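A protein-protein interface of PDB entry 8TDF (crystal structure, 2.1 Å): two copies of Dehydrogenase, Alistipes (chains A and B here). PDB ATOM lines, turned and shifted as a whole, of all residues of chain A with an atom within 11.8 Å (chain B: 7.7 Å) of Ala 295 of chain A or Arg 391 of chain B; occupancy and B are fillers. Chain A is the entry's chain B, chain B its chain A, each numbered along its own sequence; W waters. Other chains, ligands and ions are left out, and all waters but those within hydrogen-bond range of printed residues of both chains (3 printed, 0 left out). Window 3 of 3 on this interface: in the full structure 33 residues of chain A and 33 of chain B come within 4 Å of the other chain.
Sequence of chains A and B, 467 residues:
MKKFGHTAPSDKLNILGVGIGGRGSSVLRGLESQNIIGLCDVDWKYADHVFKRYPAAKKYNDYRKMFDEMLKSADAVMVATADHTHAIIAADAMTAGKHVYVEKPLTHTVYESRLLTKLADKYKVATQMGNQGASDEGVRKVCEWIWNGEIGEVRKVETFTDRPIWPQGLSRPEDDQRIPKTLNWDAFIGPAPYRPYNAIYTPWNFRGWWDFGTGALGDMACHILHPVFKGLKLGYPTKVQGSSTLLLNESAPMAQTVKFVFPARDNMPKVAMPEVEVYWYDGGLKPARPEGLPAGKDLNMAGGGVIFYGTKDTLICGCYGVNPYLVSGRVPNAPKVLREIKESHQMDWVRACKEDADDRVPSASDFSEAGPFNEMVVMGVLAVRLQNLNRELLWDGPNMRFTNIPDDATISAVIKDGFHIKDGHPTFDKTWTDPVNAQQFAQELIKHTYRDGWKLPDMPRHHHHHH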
ATOM      1  N   PHE A 160      -8.167 -13.053  21.187  1.00  0.00           N
ATOM      2  CA  PHE A 160      -7.909 -11.682  20.846  1.00  0.00           C
ATOM      3  C   PHE A 160      -8.770 -11.198  19.713  1.00  0.00           C
ATOM      4  O   PHE A 160      -9.307 -11.985  18.944  1.00  0.00           O
ATOM      5  CB  PHE A 160      -6.460 -11.505  20.380  1.00  0.00           C
ATOM      6  CG  PHE A 160      -6.205 -12.015  19.005  1.00  0.00           C
ATOM      7  CD1 PHE A 160      -6.097 -13.363  18.768  1.00  0.00           C
ATOM      8  CD2 PHE A 160      -6.004 -11.124  17.960  1.00  0.00           C
ATOM      9  CE1 PHE A 160      -5.836 -13.821  17.485  1.00  0.00           C
ATOM     10  CE2 PHE A 160      -5.782 -11.572  16.652  1.00  0.00           C
ATOM     11  CZ  PHE A 160      -5.667 -12.930  16.430  1.00  0.00           C
ATOM     12  N   LYS A 286      -1.335  -9.477  20.280  1.00  0.00           N
ATOM     13  CA  LYS A 286      -1.644 -10.845  19.938  1.00  0.00           C
ATOM     14  C   LYS A 286      -0.943 -11.790  20.899  1.00  0.00           C
ATOM     15  O   LYS A 286       0.147 -11.566  21.316  1.00  0.00           O
ATOM     16  CB  LYS A 286      -1.084 -11.220  18.576  1.00  0.00           C
ATOM     17  CG  LYS A 286      -1.714 -10.507  17.385  1.00  0.00           C
ATOM     18  CD  LYS A 286      -1.441 -11.243  16.078  1.00  0.00           C
ATOM     19  CE  LYS A 286      -1.797 -10.417  14.874  1.00  0.00           C
ATOM     20  NZ  LYS A 286      -0.984  -9.176  14.954  1.00  0.00           N
ATOM     21  N   PRO A 287      -1.519 -12.990  21.075  1.00  0.00           N
ATOM     22  CA  PRO A 287      -0.814 -14.084  21.722  1.00  0.00           C
ATOM     23  C   PRO A 287       0.356 -14.496  20.838  1.00  0.00           C
ATOM     24  O   PRO A 287       0.317 -14.307  19.601  1.00  0.00           O
ATOM     25  CB  PRO A 287      -1.856 -15.186  21.804  1.00  0.00           C
ATOM     26  CG  PRO A 287      -2.788 -14.880  20.677  1.00  0.00           C
ATOM     27  CD  PRO A 287      -2.857 -13.353  20.574  1.00  0.00           C
ATOM     28  N   ALA A 288       1.363 -15.011  21.529  1.00  0.00           N
ATOM     29  CA  ALA A 288       2.461 -15.727  20.929  1.00  0.00           C
ATOM     30  C   ALA A 288       1.935 -16.841  20.044  1.00  0.00           C
ATOM     31  O   ALA A 288       0.899 -17.425  20.344  1.00  0.00           O
ATOM     32  CB  ALA A 288       3.387 -16.249  21.992  1.00  0.00           C
ATOM     33  N   ARG A 289       2.687 -17.140  19.004  1.00  0.00           N
ATOM     34  CA  ARG A 289       2.240 -18.142  18.061  1.00  0.00           C
ATOM     35  C   ARG A 289       2.253 -19.479  18.745  1.00  0.00           C
ATOM     36  O   ARG A 289       3.212 -19.821  19.394  1.00  0.00           O
ATOM     37  CB  ARG A 289       3.116 -18.119  16.818  1.00  0.00           C
ATOM     38  CG  ARG A 289       2.723 -16.886  16.014  1.00  0.00           C
ATOM     39  CD  ARG A 289       3.309 -16.898  14.661  1.00  0.00           C
ATOM     40  NE  ARG A 289       2.795 -17.903  13.794  1.00  0.00           N
ATOM     41  CZ  ARG A 289       1.687 -17.744  13.063  1.00  0.00           C
ATOM     42  NH1 ARG A 289       0.988 -16.622  13.127  1.00  0.00           N
ATOM     43  NH2 ARG A 289       1.347 -18.678  12.211  1.00  0.00           N
ATOM     44  N   PRO A 290       1.208 -20.287  18.608  1.00  0.00           N
ATOM     45  CA  PRO A 290       1.244 -21.613  19.205  1.00  0.00           C
ATOM     46  C   PRO A 290       2.251 -22.501  18.504  1.00  0.00           C
ATOM     47  O   PRO A 290       2.388 -22.443  17.289  1.00  0.00           O
ATOM     48  CB  PRO A 290      -0.146 -22.209  18.986  1.00  0.00           C
ATOM     49  CG  PRO A 290      -0.819 -21.231  18.089  1.00  0.00           C
ATOM     50  CD  PRO A 290      -0.068 -19.937  18.020  1.00  0.00           C
ATOM     51  N   GLU A 291       2.941 -23.287  19.302  1.00  0.00           N
ATOM     52  CA  GLU A 291       3.825 -24.334  18.819  1.00  0.00           C
ATOM     53  C   GLU A 291       3.141 -25.240  17.818  1.00  0.00           C
ATOM     54  O   GLU A 291       2.024 -25.625  18.005  1.00  0.00           O
ATOM     55  CB  GLU A 291       4.301 -25.162  20.031  1.00  0.00           C
ATOM     56  CG  GLU A 291       5.671 -25.734  19.872  1.00  0.00           C
ATOM     57  CD  GLU A 291       6.687 -24.609  19.715  1.00  0.00           C
ATOM     58  OE1 GLU A 291       6.740 -23.661  20.577  1.00  0.00           O
ATOM     59  OE2 GLU A 291       7.375 -24.634  18.695  1.00  0.00           O
ATOM     60  N   GLY A 292       3.814 -25.514  16.713  1.00  0.00           N
ATOM     61  CA  GLY A 292       3.314 -26.385  15.650  1.00  0.00           C
ATOM     62  C   GLY A 292       2.567 -25.633  14.569  1.00  0.00           C
ATOM     63  O   GLY A 292       2.270 -26.213  13.557  1.00  0.00           O
ATOM     64  N   LEU A 293       2.121 -24.383  14.785  1.00  0.00           N
ATOM     65  CA  LEU A 293       1.321 -23.719  13.737  1.00  0.00           C
ATOM     66  C   LEU A 293       2.305 -23.343  12.617  1.00  0.00           C
ATOM     67  O   LEU A 293       3.393 -22.822  12.878  1.00  0.00           O
ATOM     68  CB  LEU A 293       0.638 -22.487  14.319  1.00  0.00           C
ATOM     69  CG  LEU A 293      -0.404 -21.812  13.454  1.00  0.00           C
ATOM     70  CD1 LEU A 293      -1.573 -22.749  13.226  1.00  0.00           C
ATOM     71  CD2 LEU A 293      -0.885 -20.505  14.066  1.00  0.00           C
ATOM     72  N   PRO A 294       1.989 -23.618  11.351  1.00  0.00           N
ATOM     73  CA  PRO A 294       2.886 -23.235  10.272  1.00  0.00           C
ATOM     74  C   PRO A 294       3.086 -21.709  10.272  1.00  0.00           C
ATOM     75  O   PRO A 294       2.186 -20.904  10.540  1.00  0.00           O
ATOM     76  CB  PRO A 294       2.181 -23.737   8.992  1.00  0.00           C
ATOM     77  CG  PRO A 294       1.039 -24.705   9.472  1.00  0.00           C
ATOM     78  CD  PRO A 294       0.713 -24.217  10.883  1.00  0.00           C
ATOM     79  N   ALA A 295       4.331 -21.322  10.030  1.00  0.00           N
ATOM     80  CA  ALA A 295       4.703 -19.955   9.786  1.00  0.00           C
ATOM     81  C   ALA A 295       3.762 -19.417   8.705  1.00  0.00           C
ATOM     82  O   ALA A 295       3.475 -20.109   7.746  1.00  0.00           O
ATOM     83  CB  ALA A 295       6.179 -19.900   9.363  1.00  0.00           C
ATOM     84  N   GLY A 296       3.313 -18.170   8.885  1.00  0.00           N
ATOM     85  CA  GLY A 296       2.544 -17.492   7.872  1.00  0.00           C
ATOM     86  C   GLY A 296       1.023 -17.606   8.082  1.00  0.00           C
ATOM     87  O   GLY A 296       0.253 -16.769   7.549  1.00  0.00           O
ATOM     88  N   LYS A 297       0.554 -18.646   8.784  1.00  0.00           N
ATOM     89  CA  LYS A 297      -0.885 -18.770   8.968  1.00  0.00           C
ATOM     90  C   LYS A 297      -1.343 -17.646   9.900  1.00  0.00           C
ATOM     91  O   LYS A 297      -0.902 -17.529  11.045  1.00  0.00           O
ATOM     92  CB  LYS A 297      -1.219 -20.142   9.522  1.00  0.00           C
ATOM     93  CG  LYS A 297      -2.695 -20.373   9.875  1.00  0.00           C
ATOM     94  CD  LYS A 297      -3.530 -20.581   8.672  1.00  0.00           C
ATOM     95  CE  LYS A 297      -4.751 -21.408   8.922  1.00  0.00           C
ATOM     96  NZ  LYS A 297      -5.888 -20.481   9.121  1.00  0.00           N
ATOM     97  N   ASP A 298      -2.302 -16.870   9.426  1.00  0.00           N
ATOM     98  CA  ASP A 298      -2.870 -15.784  10.157  1.00  0.00           C
ATOM     99  C   ASP A 298      -3.739 -16.328  11.284  1.00  0.00           C
ATOM    100  O   ASP A 298      -4.629 -17.132  11.053  1.00  0.00           O
ATOM    101  CB  ASP A 298      -3.556 -14.811   9.202  1.00  0.00           C
ATOM    102  CG  ASP A 298      -3.811 -13.431   9.809  1.00  0.00           C
ATOM    103  OD1 ASP A 298      -3.750 -13.278  11.105  1.00  0.00           O
ATOM    104  OD2 ASP A 298      -4.019 -12.449   9.003  1.00  0.00           O
ATOM    105  N   LEU A 299      -3.498 -15.830  12.527  1.00  0.00           N
ATOM    106  CA  LEU A 299      -4.346 -16.170  13.686  1.00  0.00           C
ATOM    107  C   LEU A 299      -5.671 -15.402  13.692  1.00  0.00           C
ATOM    108  O   LEU A 299      -6.570 -15.704  14.459  1.00  0.00           O
ATOM    109  CB  LEU A 299      -3.605 -15.799  14.969  1.00  0.00           C
ATOM    110  CG  LEU A 299      -2.484 -16.765  15.294  1.00  0.00           C
ATOM    111  CD1 LEU A 299      -1.567 -16.208  16.344  1.00  0.00           C
ATOM    112  CD2 LEU A 299      -3.094 -18.136  15.662  1.00  0.00           C
ATOM    113  N   ASN A 300      -5.731 -14.306  12.945  1.00  0.00           N
ATOM    114  CA  ASN A 300      -6.917 -13.496  12.853  1.00  0.00           C
ATOM    115  C   ASN A 300      -7.754 -14.048  11.690  1.00  0.00           C
ATOM    116  O   ASN A 300      -7.289 -14.053  10.563  1.00  0.00           O
ATOM    117  CB  ASN A 300      -6.584 -12.024  12.546  1.00  0.00           C
ATOM    118  CG  ASN A 300      -7.859 -11.209  12.449  1.00  0.00           C
ATOM    119  OD1 ASN A 300      -8.952 -11.667  11.982  1.00  0.00           O
ATOM    120  ND2 ASN A 300      -7.768  -9.996  12.953  1.00  0.00           N
ATOM    121  N   ILE A 316      -7.829 -24.146  17.167  1.00  0.00           N
ATOM    122  CA  ILE A 316      -7.818 -22.742  16.883  1.00  0.00           C
ATOM    123  C   ILE A 316      -9.070 -22.434  16.088  1.00  0.00           C
ATOM    124  O   ILE A 316      -9.349 -23.161  15.136  1.00  0.00           O
ATOM    125  CB  ILE A 316      -6.600 -22.376  16.038  1.00  0.00           C
ATOM    126  CG1 ILE A 316      -5.345 -22.692  16.808  1.00  0.00           C
ATOM    127  CG2 ILE A 316      -6.712 -20.913  15.653  1.00  0.00           C
ATOM    128  CD1 ILE A 316      -4.066 -22.219  16.103  1.00  0.00           C
ATOM    129  N   TYR A 325      -9.909 -25.518  13.346  1.00  0.00           N
ATOM    130  CA  TYR A 325      -9.004 -26.559  12.953  1.00  0.00           C
ATOM    131  C   TYR A 325      -8.103 -26.882  14.133  1.00  0.00           C
ATOM    132  O   TYR A 325      -8.008 -26.170  15.119  1.00  0.00           O
ATOM    133  CB  TYR A 325      -8.142 -26.097  11.779  1.00  0.00           C
ATOM    134  CG  TYR A 325      -7.289 -24.872  12.029  1.00  0.00           C
ATOM    135  CD1 TYR A 325      -7.831 -23.595  11.953  1.00  0.00           C
ATOM    136  CD2 TYR A 325      -5.939 -24.966  12.345  1.00  0.00           C
ATOM    137  CE1 TYR A 325      -7.049 -22.478  12.205  1.00  0.00           C
ATOM    138  CE2 TYR A 325      -5.136 -23.875  12.532  1.00  0.00           C
ATOM    139  CZ  TYR A 325      -5.683 -22.610  12.453  1.00  0.00           C
ATOM    140  OH  TYR A 325      -4.954 -21.453  12.629  1.00  0.00           O
ATOM    141  N   VAL A 327      -4.162 -27.850  15.140  1.00  0.00           N
ATOM    142  CA  VAL A 327      -2.837 -27.538  14.654  1.00  0.00           C
ATOM    143  C   VAL A 327      -2.161 -28.792  14.112  1.00  0.00           C
ATOM    144  O   VAL A 327      -1.355 -28.692  13.189  1.00  0.00           O
ATOM    145  CB  VAL A 327      -2.020 -26.900  15.766  1.00  0.00           C
ATOM    146  CG1 VAL A 327      -0.535 -26.895  15.494  1.00  0.00           C
ATOM    147  CG2 VAL A 327      -2.511 -25.505  16.027  1.00  0.00           C
ATOM    148  N   VAL B 240      12.364 -14.900  17.890  1.00  0.00           N
ATOM    149  CA  VAL B 240      11.787 -13.664  18.393  1.00  0.00           C
ATOM    150  C   VAL B 240      10.446 -13.444  17.706  1.00  0.00           C
ATOM    151  O   VAL B 240      10.285 -13.813  16.547  1.00  0.00           O
ATOM    152  CB  VAL B 240      12.776 -12.509  18.214  1.00  0.00           C
ATOM    153  CG1 VAL B 240      12.958 -12.206  16.723  1.00  0.00           C
ATOM    154  CG2 VAL B 240      12.369 -11.269  18.986  1.00  0.00           C
ATOM    155  N   GLN B 241       9.495 -12.836  18.398  1.00  0.00           N
ATOM    156  CA  GLN B 241       8.267 -12.405  17.788  1.00  0.00           C
ATOM    157  C   GLN B 241       7.698 -11.245  18.585  1.00  0.00           C
ATOM    158  O   GLN B 241       8.037 -11.069  19.765  1.00  0.00           O
ATOM    159  CB  GLN B 241       7.311 -13.572  17.677  1.00  0.00           C
ATOM    160  CG  GLN B 241       6.741 -13.952  19.061  1.00  0.00           C
ATOM    161  CD  GLN B 241       6.051 -15.265  19.001  1.00  0.00           C
ATOM    162  OE1 GLN B 241       6.676 -16.257  19.373  1.00  0.00           O
ATOM    163  NE2 GLN B 241       4.841 -15.269  18.465  1.00  0.00           N
ATOM    164  N   GLY B 242       6.920 -10.393  17.924  1.00  0.00           N
ATOM    165  CA  GLY B 242       6.331  -9.263  18.583  1.00  0.00           C
ATOM    166  C   GLY B 242       4.939  -8.929  18.073  1.00  0.00           C
ATOM    167  O   GLY B 242       4.611  -9.251  16.910  1.00  0.00           O
ATOM    168  N   ALA B 383      11.410  -7.351  15.571  1.00  0.00           N
ATOM    169  CA  ALA B 383      10.263  -8.199  15.750  1.00  0.00           C
ATOM    170  C   ALA B 383       8.985  -7.425  15.544  1.00  0.00           C
ATOM    171  O   ALA B 383       8.024  -7.947  15.032  1.00  0.00           O
ATOM    172  CB  ALA B 383      10.285  -8.807  17.093  1.00  0.00           C
ATOM    173  N   LEU B 386       8.269  -6.374  11.900  1.00  0.00           N
ATOM    174  CA  LEU B 386       8.032  -7.536  11.054  1.00  0.00           C
ATOM    175  C   LEU B 386       6.795  -8.328  11.440  1.00  0.00           C
ATOM    176  O   LEU B 386       6.587  -9.404  10.938  1.00  0.00           O
ATOM    177  CB  LEU B 386       9.265  -8.399  11.050  1.00  0.00           C
ATOM    178  CG  LEU B 386      10.511  -7.704  10.452  1.00  0.00           C
ATOM    179  CD1 LEU B 386      11.763  -8.514  10.678  1.00  0.00           C
ATOM    180  CD2 LEU B 386      10.328  -7.551   8.988  1.00  0.00           C
ATOM    181  N   GLN B 387       5.981  -7.811  12.326  1.00  0.00           N
ATOM    182  CA  GLN B 387       4.936  -8.638  12.891  1.00  0.00           C
ATOM    183  C   GLN B 387       3.933  -9.046  11.802  1.00  0.00           C
ATOM    184  O   GLN B 387       3.251 -10.028  11.996  1.00  0.00           O
ATOM    185  CB  GLN B 387       4.144  -7.862  13.963  1.00  0.00           C
ATOM    186  CG  GLN B 387       3.476  -6.559  13.434  1.00  0.00           C
ATOM    187  CD  GLN B 387       2.850  -5.754  14.533  1.00  0.00           C
ATOM    188  OE1 GLN B 387       1.721  -5.952  14.885  1.00  0.00           O
ATOM    189  NE2 GLN B 387       3.613  -4.961  15.247  1.00  0.00           N
ATOM    190  N   ASN B 388       3.793  -8.325  10.669  1.00  0.00           N
ATOM    191  CA  ASN B 388       2.763  -8.745   9.708  1.00  0.00           C
ATOM    192  C   ASN B 388       3.136 -10.056   9.031  1.00  0.00           C
ATOM    193  O   ASN B 388       2.338 -10.591   8.271  1.00  0.00           O
ATOM    194  CB  ASN B 388       2.530  -7.701   8.608  1.00  0.00           C
ATOM    195  CG  ASN B 388       1.856  -6.472   9.183  1.00  0.00           C
ATOM    196  OD1 ASN B 388       1.351  -6.490  10.320  1.00  0.00           O
ATOM    197  ND2 ASN B 388       1.731  -5.451   8.334  1.00  0.00           N
ATOM    198  N   LEU B 389       4.406 -10.495   9.159  1.00  0.00           N
ATOM    199  CA  LEU B 389       4.770 -11.804   8.594  1.00  0.00           C
ATOM    200  C   LEU B 389       4.083 -12.988   9.291  1.00  0.00           C
ATOM    201  O   LEU B 389       4.129 -14.108   8.782  1.00  0.00           O
ATOM    202  CB  LEU B 389       6.273 -11.965   8.729  1.00  0.00           C
ATOM    203  CG  LEU B 389       7.078 -11.019   7.834  1.00  0.00           C
ATOM    204  CD1 LEU B 389       8.556 -11.122   8.094  1.00  0.00           C
ATOM    205  CD2 LEU B 389       6.725 -11.256   6.367  1.00  0.00           C
ATOM    206  N   ASN B 390       3.481 -12.828  10.496  1.00  0.00           N
ATOM    207  CA  ASN B 390       2.667 -13.930  11.024  1.00  0.00           C
ATOM    208  C   ASN B 390       3.500 -15.180  11.245  1.00  0.00           C
ATOM    209  O   ASN B 390       3.091 -16.279  10.885  1.00  0.00           O
ATOM    210  CB  ASN B 390       1.407 -14.226  10.210  1.00  0.00           C
ATOM    211  CG  ASN B 390       0.421 -13.081  10.357  1.00  0.00           C
ATOM    212  OD1 ASN B 390       0.477 -12.289  11.310  1.00  0.00           O
ATOM    213  ND2 ASN B 390      -0.403 -12.911   9.365  1.00  0.00           N
ATOM    214  N   ARG B 391       4.670 -14.997  11.886  1.00  0.00           N
ATOM    215  CA  ARG B 391       5.543 -16.118  12.139  1.00  0.00           C
ATOM    216  C   ARG B 391       6.466 -15.724  13.279  1.00  0.00           C
ATOM    217  O   ARG B 391       6.649 -14.534  13.524  1.00  0.00           O
ATOM    218  CB  ARG B 391       6.384 -16.507  10.942  1.00  0.00           C
ATOM    219  CG  ARG B 391       7.272 -15.405  10.385  1.00  0.00           C
ATOM    220  CD  ARG B 391       8.003 -15.765   9.079  1.00  0.00           C
ATOM    221  NE  ARG B 391       6.967 -16.018   8.092  1.00  0.00           N
ATOM    222  CZ  ARG B 391       6.968 -17.040   7.291  1.00  0.00           C
ATOM    223  NH1 ARG B 391       7.986 -17.894   7.264  1.00  0.00           N
ATOM    224  NH2 ARG B 391       5.877 -17.234   6.612  1.00  0.00           N
ATOM    225  N   GLU B 392       6.935 -16.760  13.983  1.00  0.00           N
ATOM    226  CA  GLU B 392       8.002 -16.605  14.946  1.00  0.00           C
ATOM    227  C   GLU B 392       9.257 -16.514  14.119  1.00  0.00           C
ATOM    228  O   GLU B 392       9.413 -17.368  13.314  1.00  0.00           O
ATOM    229  CB  GLU B 392       7.996 -17.819  15.875  1.00  0.00           C
ATOM    230  CG  GLU B 392       9.078 -17.740  16.927  1.00  0.00           C
ATOM    231  CD  GLU B 392       9.038 -18.868  18.002  1.00  0.00           C
ATOM    232  OE1 GLU B 392       8.881 -20.102  17.548  1.00  0.00           O
ATOM    233  OE2 GLU B 392       9.260 -18.539  19.260  1.00  0.00           O
ATOM    234  N   LEU B 393      10.057 -15.470  14.203  1.00  0.00           N
ATOM    235  CA  LEU B 393      11.266 -15.337  13.359  1.00  0.00           C
ATOM    236  C   LEU B 393      12.444 -16.113  13.971  1.00  0.00           C
ATOM    237  O   LEU B 393      12.628 -16.100  15.199  1.00  0.00           O
ATOM    238  CB  LEU B 393      11.644 -13.872  13.253  1.00  0.00           C
ATOM    239  CG  LEU B 393      10.505 -12.994  12.698  1.00  0.00           C
ATOM    240  CD1 LEU B 393      10.678 -11.539  13.027  1.00  0.00           C
ATOM    241  CD2 LEU B 393      10.453 -13.143  11.251  1.00  0.00           C
ATOM    242  N   LEU B 394      13.197 -16.831  13.141  1.00  0.00           N
ATOM    243  CA  LEU B 394      14.345 -17.587  13.588  1.00  0.00           C
ATOM    244  C   LEU B 394      15.574 -16.770  13.267  1.00  0.00           C
ATOM    245  O   LEU B 394      15.766 -16.372  12.083  1.00  0.00           O
ATOM    246  CB  LEU B 394      14.309 -18.959  12.895  1.00  0.00           C
ATOM    247  CG  LEU B 394      13.020 -19.789  13.122  1.00  0.00           C
ATOM    248  CD1 LEU B 394      13.039 -21.172  12.460  1.00  0.00           C
ATOM    249  CD2 LEU B 394      12.799 -20.037  14.591  1.00  0.00           C
ATOM    250  N   THR B 403      16.391 -16.544   9.251  1.00  0.00           N
ATOM    251  CA  THR B 403      16.527 -17.677   8.366  1.00  0.00           C
ATOM    252  C   THR B 403      15.173 -18.116   7.772  1.00  0.00           C
ATOM    253  O   THR B 403      15.175 -18.982   6.891  1.00  0.00           O
ATOM    254  CB  THR B 403      17.091 -18.906   9.099  1.00  0.00           C
ATOM    255  OG1 THR B 403      16.166 -19.327  10.116  1.00  0.00           O
ATOM    256  CG2 THR B 403      18.425 -18.651   9.743  1.00  0.00           C
ATOM    257  N   ASN B 404      14.020 -17.595   8.243  1.00  0.00           N
ATOM    258  CA  ASN B 404      12.749 -18.152   7.746  1.00  0.00           C
ATOM    259  C   ASN B 404      11.826 -17.015   7.253  1.00  0.00           C
ATOM    260  O   ASN B 404      10.611 -17.070   7.468  1.00  0.00           O
ATOM    261  CB  ASN B 404      12.037 -18.950   8.841  1.00  0.00           C
ATOM    262  CG  ASN B 404      11.668 -18.067  10.005  1.00  0.00           C
ATOM    263  OD1 ASN B 404      12.317 -17.056  10.318  1.00  0.00           O
ATOM    264  ND2 ASN B 404      10.609 -18.417  10.712  1.00  0.00           N
ATOM    265  N   ILE B 405      12.357 -15.952   6.663  1.00  0.00           N
ATOM    266  CA  ILE B 405      11.530 -15.021   5.914  1.00  0.00           C
ATOM    267  C   ILE B 405      11.451 -15.478   4.472  1.00  0.00           C
ATOM    268  O   ILE B 405      12.495 -15.541   3.839  1.00  0.00           O
ATOM    269  CB  ILE B 405      12.061 -13.593   5.955  1.00  0.00           C
ATOM    270  CG1 ILE B 405      12.167 -13.124   7.400  1.00  0.00           C
ATOM    271  CG2 ILE B 405      11.260 -12.663   5.067  1.00  0.00           C
ATOM    272  CD1 ILE B 405      12.749 -11.792   7.544  1.00  0.00           C
ATOM    273  N   PRO B 406      10.263 -15.855   3.941  1.00  0.00           N
ATOM    274  CA  PRO B 406      10.114 -16.270   2.548  1.00  0.00           C
ATOM    275  C   PRO B 406      10.621 -15.212   1.574  1.00  0.00           C
ATOM    276  O   PRO B 406      10.483 -14.008   1.788  1.00  0.00           O
ATOM    277  CB  PRO B 406       8.613 -16.531   2.300  1.00  0.00           C
ATOM    278  CG  PRO B 406       8.022 -16.602   3.718  1.00  0.00           C
ATOM    279  CD  PRO B 406       8.973 -15.843   4.633  1.00  0.00           C
ATOM    280  N   ALA B 409       7.795 -12.853   0.336  1.00  0.00           N
ATOM    281  CA  ALA B 409       6.884 -12.221   1.268  1.00  0.00           C
ATOM    282  C   ALA B 409       7.056 -10.722   1.230  1.00  0.00           C
ATOM    283  O   ALA B 409       8.093 -10.244   0.870  1.00  0.00           O
ATOM    284  CB  ALA B 409       7.186 -12.716   2.705  1.00  0.00           C
HETATM  285  O   HOH W   1      -0.365 -14.433   7.272  1.00  0.00           O
HETATM  286  O   HOH W   2       5.737 -18.778  19.630  1.00  0.00           O
HETATM  287  O   HOH W   3      -1.413 -13.994  12.983  1.00  0.00           O
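NE2 of Gln 241 of chain B sits close to N of Arg 289 of chain A.
The guanidinium group (NH1) of Arg 289 of chain A sits close to the backbone carbonyl oxygen (O) of Asn 390 of chain B (3.1 Å).
The backbone NH (N) of Gly 296 of chain A sits at hydrogen-bond distance from the backbone carbonyl oxygen (O) of Asn 390 of chain B (2.8 Å).
No position is printed for both chains.
Of the 11 pairs that touch across the chains among the printed residues, none has its exchanged pair printed and touching as well.
The backbone carbonyl oxygen (O) of Glu 392 of chain B lies within hydrogen-bond range of the side-chain amide nitrogen (ND2) of Asn 404 of chain B.
The backbone NH (N) of Asn 300 of chain A sits at hydrogen-bond distance from the side-chain carboxylate (OD1) of Asp 298 of chain A (2.9 Å).
The guanidinium group (NH1) of Arg 391 of chain B lies within hydrogen-bond range of the backbone carbonyl oxygen (O) of Asn 404 of chain B.
OE2 of Glu 392 of chain B lies close to OE1 of Gln 241 of chain B (3.4 Å).
O of Leu 389 of chain B sits at hydrogen-bond distance from NE of Arg 391 of chain B (3.5 Å).
O of Pro 294 of chain A sits at hydrogen-bond distance from NH2 of Arg 289 of chain A.
Among the printed residues, merely in contact across the chains: Ala 295 of chain A with Arg 391 of chain B (3.4 Å), Ala 288 of chain A with Gln 241 of chain B (3.5 Å), Arg 289 of chain A with Arg 391 of chain B (3.5 Å), Asp 298 of chain A with Asn 390 of chain B (3.5 Å), Gly 296 of chain A with Arg 391 of chain B (3.6 Å), Arg 289 of chain A with Glu 392 of chain B (3.7 Å), Gly 296 of chain A with Leu 389 of chain B (3.8 Å) and Ala 295 of chain A with Asn 390 of chain B (3.9 Å).
Hydrophobic or aromatic side chains of chain A within 4 Å of the printed part of chain B: Ala 288 and Ala 295.
Of the 18 printed residues of chain B, 5 touch a printed residue of chain A.
Among the printed residues, 11 pairs touch across the chains.
Ala 295 of chain A touches two residues of chain B.
Of chain A, only Arg 289 (3.5 Å), Ala 295 (3.4 Å) and Gly 296 (3.6 Å) come within 4 Å of Arg 391 of chain B.
Of chain A, only Ala 288 (3.5 Å) and Arg 289 (2.9 Å) come within 4 Å of Gln 241 of chain B.
No residue of chain A comes within 4 Å of Gly 242 of chain B.
Of chain A, only Gly 296 comes within 4 Å of Leu 389 of chain B.
Asn 390 of chain B touches just these residues of chain A: Arg 289 (3.0 Å), Ala 295 (3.9 Å), Gly 296 (2.8 Å) and Asp 298 (3.5 Å).
Glu 392 of chain B touches just one residue of chain A: Arg 289 (3.7 Å).
No residue of chain A comes within 4 Å of Leu 393 of chain B.
No residue of chain A comes within 4 Å of Asn 404 of chain B.
No residue of chain A comes within 4 Å of Ile 405 of chain B.
Of the printed residues of chain B, Ala 288 of chain A touches Gln 241.
Of the printed residues of chain B, Gly 296 of chain A touches Leu 389 (3.8 Å), Asn 390 (2.8 Å) and Arg 391 (3.6 Å).
Printed residues of chain B within 4 Å of Arg 289 of chain A: Gln 241 (2.9 Å), Asn 390 (3.0 Å), Arg 391 (3.5 Å) and Glu 392 (3.7 Å).
Of the printed residues of chain B, Asp 298 of chain A touches Asn 390.
Gly 292 of chain A touches none of the printed residues of chain B.
The nearest residue of chain B that does not touch Ala 295 of chain A is Asn 404 of chain B (4.9 Å).
The nearest residue of chain A that does not touch Arg 391 of chain B is Lys 297 of chain A (5.9 Å).
Water W1 bridges O of Gly 296 of chain A (2.4 Å) and ND2 of Asn 390 of chain B (2.6 Å).
Water W2 bridges OE1 of Gln 241 of chain B (2.7 Å) and O of Arg 289 of chain A (2.7 Å).
Water W3 lies within hydrogen-bond range of the backbone NH of Leu 299 of chain A (2.8 Å), the side-chain amide oxygen of Asn 390 of chain B (3.0 Å) and the side-chain carboxylate of Asp 298 of chain A (3.1 Å).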
